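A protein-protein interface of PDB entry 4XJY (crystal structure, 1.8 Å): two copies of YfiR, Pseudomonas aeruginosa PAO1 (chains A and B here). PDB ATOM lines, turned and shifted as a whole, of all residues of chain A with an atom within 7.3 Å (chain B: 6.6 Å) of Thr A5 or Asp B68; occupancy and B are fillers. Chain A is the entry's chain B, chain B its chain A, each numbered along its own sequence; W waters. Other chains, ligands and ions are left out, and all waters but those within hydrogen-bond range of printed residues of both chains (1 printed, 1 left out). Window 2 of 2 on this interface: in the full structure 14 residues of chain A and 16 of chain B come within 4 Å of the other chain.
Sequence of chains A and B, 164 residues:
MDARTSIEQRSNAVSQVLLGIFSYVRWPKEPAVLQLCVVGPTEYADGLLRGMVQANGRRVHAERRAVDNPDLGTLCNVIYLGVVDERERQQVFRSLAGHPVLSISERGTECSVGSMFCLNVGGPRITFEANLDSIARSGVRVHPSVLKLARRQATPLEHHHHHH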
ATOM      1  N   ARG A   4      -0.658 -13.860 -12.184  1.00  0.00           N
ATOM      2  CA  ARG A   4      -1.233 -15.179 -12.434  1.00  0.00           C
ATOM      3  C   ARG A   4      -1.082 -15.598 -13.895  1.00  0.00           C
ATOM      4  O   ARG A   4      -1.214 -14.769 -14.805  1.00  0.00           O
ATOM      5  CB  ARG A   4      -2.717 -15.211 -12.057  1.00  0.00           C
ATOM      6  CG  ARG A   4      -3.045 -14.909 -10.590  1.00  0.00           C
ATOM      7  CD  ARG A   4      -2.725 -16.077  -9.664  1.00  0.00           C
ATOM      8  NE  ARG A   4      -3.181 -15.793  -8.309  1.00  0.00           N
ATOM      9  CZ  ARG A   4      -4.409 -16.050  -7.863  1.00  0.00           C
ATOM     10  NH1 ARG A   4      -5.321 -16.592  -8.669  1.00  0.00           N
ATOM     11  NH2 ARG A   4      -4.730 -15.757  -6.606  1.00  0.00           N
ATOM     12  N   THR A   5      -0.835 -16.891 -14.095  1.00  0.00           N
ATOM     13  CA  THR A   5      -0.844 -17.528 -15.415  1.00  0.00           C
ATOM     14  C   THR A   5      -2.173 -17.395 -16.159  1.00  0.00           C
ATOM     15  O   THR A   5      -3.241 -17.749 -15.625  1.00  0.00           O
ATOM     16  CB  THR A   5      -0.523 -19.038 -15.305  1.00  0.00           C
ATOM     17  OG1 THR A   5       0.803 -19.207 -14.798  1.00  0.00           O
ATOM     18  CG2 THR A   5      -0.620 -19.740 -16.679  1.00  0.00           C
ATOM     19  N   SER A   6      -2.106 -16.872 -17.384  1.00  0.00           N
ATOM     20  CA  SER A   6      -3.282 -16.798 -18.222  1.00  0.00           C
ATOM     21  C   SER A   6      -3.177 -17.799 -19.355  1.00  0.00           C
ATOM     22  O   SER A   6      -2.340 -17.636 -20.268  1.00  0.00           O
ATOM     23  CB  SER A   6      -3.466 -15.405 -18.807  1.00  0.00           C
ATOM     24  OG  SER A   6      -4.570 -15.404 -19.697  1.00  0.00           O
ATOM     25  N   ILE A   7      -4.039 -18.815 -19.326  1.00  0.00           N
ATOM     26  CA  ILE A   7      -4.033 -19.815 -20.391  1.00  0.00           C
ATOM     27  C   ILE A   7      -4.490 -19.148 -21.703  1.00  0.00           C
ATOM     28  O   ILE A   7      -3.953 -19.424 -22.782  1.00  0.00           O
ATOM     29  CB  ILE A   7      -4.920 -21.023 -20.087  1.00  0.00           C
ATOM     30  CG1 ILE A   7      -4.386 -21.797 -18.863  1.00  0.00           C
ATOM     31  CG2 ILE A   7      -4.880 -21.980 -21.258  1.00  0.00           C
ATOM     32  CD1 ILE A   7      -2.985 -22.353 -19.071  1.00  0.00           C
ATOM     33  N   GLU A   8      -5.464 -18.249 -21.603  1.00  0.00           N
ATOM     34  CA  GLU A   8      -5.950 -17.510 -22.765  1.00  0.00           C
ATOM     35  C   GLU A   8      -4.883 -16.644 -23.429  1.00  0.00           C
ATOM     36  O   GLU A   8      -4.671 -16.695 -24.659  1.00  0.00           O
ATOM     37  CB  GLU A   8      -7.104 -16.605 -22.338  1.00  0.00           C
ATOM     38  CG  GLU A   8      -7.717 -15.835 -23.490  1.00  0.00           C
ATOM     39  CD  GLU A   8      -8.763 -14.808 -23.042  1.00  0.00           C
ATOM     40  OE1 GLU A   8      -9.095 -14.737 -21.835  1.00  0.00           O
ATOM     41  OE2 GLU A   8      -9.272 -14.084 -23.925  1.00  0.00           O
ATOM     42  N   GLN A   9      -4.154 -15.891 -22.622  1.00  0.00           N
ATOM     43  CA  GLN A   9      -3.111 -15.053 -23.197  1.00  0.00           C
ATOM     44  C   GLN A   9      -2.014 -15.883 -23.821  1.00  0.00           C
ATOM     45  O   GLN A   9      -1.517 -15.549 -24.919  1.00  0.00           O
ATOM     46  CB  GLN A   9      -2.527 -14.106 -22.156  1.00  0.00           C
ATOM     47  CG  GLN A   9      -3.483 -12.971 -21.814  1.00  0.00           C
ATOM     48  CD  GLN A   9      -2.842 -11.916 -20.934  1.00  0.00           C
ATOM     49  OE1 GLN A   9      -1.727 -12.101 -20.434  1.00  0.00           O
ATOM     50  NE2 GLN A   9      -3.517 -10.780 -20.781  1.00  0.00           N
ATOM     51  N   ARG A  10      -1.646 -16.968 -23.157  1.00  0.00           N
ATOM     52  CA  ARG A  10      -0.588 -17.826 -23.697  1.00  0.00           C
ATOM     53  C   ARG A  10      -1.042 -18.487 -24.981  1.00  0.00           C
ATOM     54  O   ARG A  10      -0.245 -18.637 -25.901  1.00  0.00           O
ATOM     55  CB  ARG A  10      -0.182 -18.904 -22.690  1.00  0.00           C
ATOM     56  CG  ARG A  10       0.508 -18.330 -21.455  1.00  0.00           C
ATOM     57  CD  ARG A  10       0.962 -19.427 -20.543  1.00  0.00           C
ATOM     58  NE  ARG A  10       1.801 -18.907 -19.471  1.00  0.00           N
ATOM     59  CZ  ARG A  10       2.432 -19.679 -18.599  1.00  0.00           C
ATOM     60  NH1 ARG A  10       2.313 -20.994 -18.687  1.00  0.00           N
ATOM     61  NH2 ARG A  10       3.182 -19.139 -17.647  1.00  0.00           N
ATOM     62  N   GLU A  43      -2.021 -27.959 -24.379  1.00  0.00           N
ATOM     63  CA  GLU A  43      -2.657 -27.013 -23.476  1.00  0.00           C
ATOM     64  C   GLU A  43      -2.971 -25.685 -24.159  1.00  0.00           C
ATOM     65  O   GLU A  43      -3.906 -24.990 -23.753  1.00  0.00           O
ATOM     66  CB  GLU A  43      -1.750 -26.767 -22.287  1.00  0.00           C
ATOM     67  CG  GLU A  43      -2.369 -26.004 -21.159  1.00  0.00           C
ATOM     68  CD  GLU A  43      -1.572 -26.145 -19.877  1.00  0.00           C
ATOM     69  OE1 GLU A  43      -0.433 -26.678 -19.939  1.00  0.00           O
ATOM     70  OE2 GLU A  43      -2.088 -25.721 -18.822  1.00  0.00           O
ATOM     71  N   TYR A  44      -2.166 -25.323 -25.170  1.00  0.00           N
ATOM     72  CA  TYR A  44      -2.189 -23.964 -25.721  1.00  0.00           C
ATOM     73  C   TYR A  44      -2.665 -23.903 -27.174  1.00  0.00           C
ATOM     74  O   TYR A  44      -2.484 -22.879 -27.852  1.00  0.00           O
ATOM     75  CB  TYR A  44      -0.781 -23.340 -25.602  1.00  0.00           C
ATOM     76  CG  TYR A  44      -0.315 -23.234 -24.173  1.00  0.00           C
ATOM     77  CD1 TYR A  44      -0.980 -22.399 -23.287  1.00  0.00           C
ATOM     78  CD2 TYR A  44       0.714 -24.042 -23.676  1.00  0.00           C
ATOM     79  CE1 TYR A  44      -0.600 -22.306 -21.964  1.00  0.00           C
ATOM     80  CE2 TYR A  44       1.107 -23.960 -22.333  1.00  0.00           C
ATOM     81  CZ  TYR A  44       0.445 -23.086 -21.494  1.00  0.00           C
ATOM     82  OH  TYR A  44       0.801 -22.957 -20.167  1.00  0.00           O
ATOM     83  N   GLY A 123       7.021 -18.486 -18.476  1.00  0.00           N
ATOM     84  CA  GLY A 123       7.794 -17.270 -18.324  1.00  0.00           C
ATOM     85  C   GLY A 123       7.003 -16.056 -18.750  1.00  0.00           C
ATOM     86  O   GLY A 123       5.799 -16.149 -18.986  1.00  0.00           O
ATOM     87  N   VAL B  39      -7.694 -28.846 -17.222  1.00  0.00           N
ATOM     88  CA  VAL B  39      -6.425 -28.378 -16.695  1.00  0.00           C
ATOM     89  C   VAL B  39      -5.285 -29.224 -17.253  1.00  0.00           C
ATOM     90  O   VAL B  39      -5.264 -30.445 -17.073  1.00  0.00           O
ATOM     91  CB  VAL B  39      -6.445 -28.384 -15.144  1.00  0.00           C
ATOM     92  CG1 VAL B  39      -5.097 -27.992 -14.527  1.00  0.00           C
ATOM     93  CG2 VAL B  39      -7.549 -27.421 -14.641  1.00  0.00           C
ATOM     94  N   ARG B  65      -8.284 -23.895 -17.447  1.00  0.00           N
ATOM     95  CA  ARG B  65      -7.607 -23.149 -16.390  1.00  0.00           C
ATOM     96  C   ARG B  65      -6.202 -23.688 -16.152  1.00  0.00           C
ATOM     97  O   ARG B  65      -5.850 -24.797 -16.583  1.00  0.00           O
ATOM     98  CB  ARG B  65      -8.429 -23.179 -15.091  1.00  0.00           C
ATOM     99  CG  ARG B  65      -9.820 -22.558 -15.250  1.00  0.00           C
ATOM    100  CD  ARG B  65     -10.451 -22.199 -13.921  1.00  0.00           C
ATOM    101  NE  ARG B  65     -11.832 -21.690 -14.015  1.00  0.00           N
ATOM    102  CZ  ARG B  65     -12.164 -20.455 -14.396  1.00  0.00           C
ATOM    103  NH1 ARG B  65     -11.224 -19.601 -14.799  1.00  0.00           N
ATOM    104  NH2 ARG B  65     -13.451 -20.071 -14.418  1.00  0.00           N
ATOM    105  N   ALA B  66      -5.388 -22.863 -15.503  1.00  0.00           N
ATOM    106  CA  ALA B  66      -3.981 -23.182 -15.279  1.00  0.00           C
ATOM    107  C   ALA B  66      -3.757 -24.139 -14.112  1.00  0.00           C
ATOM    108  O   ALA B  66      -4.453 -24.105 -13.096  1.00  0.00           O
ATOM    109  CB  ALA B  66      -3.188 -21.900 -15.059  1.00  0.00           C
ATOM    110  N   VAL B  67      -2.744 -24.982 -14.264  1.00  0.00           N
ATOM    111  CA  VAL B  67      -2.340 -25.893 -13.205  1.00  0.00           C
ATOM    112  C   VAL B  67      -2.049 -25.158 -11.914  1.00  0.00           C
ATOM    113  O   VAL B  67      -2.366 -25.663 -10.827  1.00  0.00           O
ATOM    114  CB  VAL B  67      -1.075 -26.675 -13.626  1.00  0.00           C
ATOM    115  CG1 VAL B  67      -0.410 -27.326 -12.391  1.00  0.00           C
ATOM    116  CG2 VAL B  67      -1.455 -27.713 -14.668  1.00  0.00           C
ATOM    117  N   ASP B  68      -1.482 -23.955 -12.028  1.00  0.00           N
ATOM    118  CA  ASP B  68      -1.060 -23.217 -10.840  1.00  0.00           C
ATOM    119  C   ASP B  68      -2.081 -22.183 -10.393  1.00  0.00           C
ATOM    120  O   ASP B  68      -1.802 -21.362  -9.527  1.00  0.00           O
ATOM    121  CB  ASP B  68       0.300 -22.547 -11.087  1.00  0.00           C
ATOM    122  CG  ASP B  68       0.262 -21.515 -12.212  1.00  0.00           C
ATOM    123  OD1 ASP B  68      -0.789 -21.377 -12.883  1.00  0.00           O
ATOM    124  OD2 ASP B  68       1.297 -20.841 -12.433  1.00  0.00           O
ATOM    125  N   ASN B  69      -3.294 -22.262 -10.917  1.00  0.00           N
ATOM    126  CA  ASN B  69      -4.349 -21.396 -10.410  1.00  0.00           C
ATOM    127  C   ASN B  69      -4.697 -21.867  -9.001  1.00  0.00           C
ATOM    128  O   ASN B  69      -5.187 -22.979  -8.837  1.00  0.00           O
ATOM    129  CB  ASN B  69      -5.590 -21.436 -11.316  1.00  0.00           C
ATOM    130  CG  ASN B  69      -6.650 -20.421 -10.907  1.00  0.00           C
ATOM    131  OD1 ASN B  69      -6.802 -20.102  -9.731  1.00  0.00           O
ATOM    132  ND2 ASN B  69      -7.387 -19.913 -11.872  1.00  0.00           N
ATOM    133  N   PRO B  70      -4.411 -21.039  -7.986  1.00  0.00           N
ATOM    134  CA  PRO B  70      -4.644 -21.450  -6.596  1.00  0.00           C
ATOM    135  C   PRO B  70      -6.118 -21.606  -6.250  1.00  0.00           C
ATOM    136  O   PRO B  70      -6.403 -22.174  -5.206  1.00  0.00           O
ATOM    137  CB  PRO B  70      -4.034 -20.302  -5.787  1.00  0.00           C
ATOM    138  CG  PRO B  70      -4.149 -19.125  -6.683  1.00  0.00           C
ATOM    139  CD  PRO B  70      -3.854 -19.677  -8.059  1.00  0.00           C
ATOM    140  N   ASP B  71      -7.029 -21.120  -7.093  1.00  0.00           N
ATOM    141  CA  ASP B  71      -8.446 -21.151  -6.772  1.00  0.00           C
ATOM    142  C   ASP B  71      -9.207 -22.244  -7.495  1.00  0.00           C
ATOM    143  O   ASP B  71     -10.422 -22.202  -7.520  1.00  0.00           O
ATOM    144  CB  ASP B  71      -9.095 -19.804  -7.092  1.00  0.00           C
ATOM    145  CG  ASP B  71      -8.453 -18.659  -6.336  1.00  0.00           C
ATOM    146  OD1 ASP B  71      -8.146 -18.837  -5.151  1.00  0.00           O
ATOM    147  OD2 ASP B  71      -8.234 -17.584  -6.935  1.00  0.00           O
ATOM    148  N   LEU B  72      -8.516 -23.236  -8.064  1.00  0.00           N
ATOM    149  CA  LEU B  72      -9.241 -24.314  -8.747  1.00  0.00           C
ATOM    150  C   LEU B  72     -10.351 -24.926  -7.873  1.00  0.00           C
ATOM    151  O   LEU B  72     -11.460 -25.223  -8.354  1.00  0.00           O
ATOM    152  CB  LEU B  72      -8.265 -25.418  -9.184  1.00  0.00           C
ATOM    153  CG  LEU B  72      -7.257 -24.997 -10.249  1.00  0.00           C
ATOM    154  CD1 LEU B  72      -6.358 -26.211 -10.585  1.00  0.00           C
ATOM    155  CD2 LEU B  72      -7.944 -24.416 -11.492  1.00  0.00           C
ATOM    156  N   GLN B  91       0.460 -30.136  -7.198  1.00  0.00           N
ATOM    157  CA  GLN B  91      -0.010 -28.751  -7.058  1.00  0.00           C
ATOM    158  C   GLN B  91      -1.522 -28.640  -7.275  1.00  0.00           C
ATOM    159  O   GLN B  91      -2.237 -27.962  -6.501  1.00  0.00           O
ATOM    160  CB  GLN B  91       0.719 -27.818  -8.036  1.00  0.00           C
ATOM    161  CG  GLN B  91       0.320 -26.346  -7.884  1.00  0.00           C
ATOM    162  CD  GLN B  91       1.236 -25.396  -8.660  1.00  0.00           C
ATOM    163  OE1 GLN B  91       1.902 -25.794  -9.622  1.00  0.00           O
ATOM    164  NE2 GLN B  91       1.280 -24.134  -8.234  1.00  0.00           N
ATOM    165  N   VAL B  92      -2.024 -29.305  -8.315  1.00  0.00           N
ATOM    166  CA  VAL B  92      -3.471 -29.325  -8.524  1.00  0.00           C
ATOM    167  C   VAL B  92      -4.212 -29.882  -7.310  1.00  0.00           C
ATOM    168  O   VAL B  92      -5.170 -29.276  -6.817  1.00  0.00           O
ATOM    169  CB  VAL B  92      -3.885 -30.153  -9.765  1.00  0.00           C
ATOM    170  CG1 VAL B  92      -5.421 -30.307  -9.790  1.00  0.00           C
ATOM    171  CG2 VAL B  92      -3.397 -29.481 -11.061  1.00  0.00           C
ATOM    172  N   SER B  95      -4.506 -27.776  -4.275  1.00  0.00           N
ATOM    173  CA  SER B  95      -5.527 -26.752  -4.474  1.00  0.00           C
ATOM    174  C   SER B  95      -6.943 -27.273  -4.271  1.00  0.00           C
ATOM    175  O   SER B  95      -7.826 -26.526  -3.849  1.00  0.00           O
ATOM    176  CB  SER B  95      -5.400 -26.142  -5.875  1.00  0.00           C
ATOM    177  OG  SER B  95      -4.138 -25.509  -6.001  1.00  0.00           O
HETATM  178  O   HOH W   1      -4.928 -25.835 -18.967  1.00  0.00           O
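Of the 10 printed residues of chain A, 3 touch a printed residue of chain B. Printed residues of chain A that touch a printed residue of chain B: Arg A4, Thr A5 and Ile A7. Hydrophobic or aromatic side chains of chain A that line the printed part of chain B: Ile A7. Printed residues of chain B that touch a printed residue of chain A: Arg B65, Ala B66, Asp B68, Asn B69, Pro B70 and Asp B71. Among the printed residues, 7 pairs touch across the chains.
Thr A5 touches just these residues of chain B: Ala B66 and Asp B68. Glu A8 touches none of the printed residues of chain B. Of the printed residues of chain A, Ala B66 touches Thr A5 and Ile A7. Val B67 touches none of the printed residues of chain A. Of the printed residues of chain A, Pro B70 touches Arg A4 (3.3 Å). The nearest printed residue of chain B that does not touch Arg A4 is Asp B68 (5.4 Å).
The side-chain carboxylate of Asp B68 is in hydrogen-bond range of the side-chain hydroxyl of Thr A5, at 2.9 Å. The guanidinium group (NH1) of Arg A4 lies within salt-bridge range of the side-chain carboxylate (OD2) of Asp B71 (3.5 Å).
No position is printed for both chains.
The side-chain amide oxygen (OD1) of Asn B69 sits at hydrogen-bond distance from the backbone NH (N) of Asp B71 (2.8 Å).
Among the printed residues, merely in contact across the chains: Arg A4 with Asn B69 (3.95 Å), Arg A4 with Pro B70 (3.3 Å), Thr A5 with Ala B66 (3.7 Å), Ile A7 with Arg B65 (3.8 Å) and Ile A7 with Ala B66 (3.7 Å).
Water W1 bridges the backbone carbonyl oxygen of Arg B65 (2.8 Å) and the side-chain carboxylate of Glu A43 (2.8 Å).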
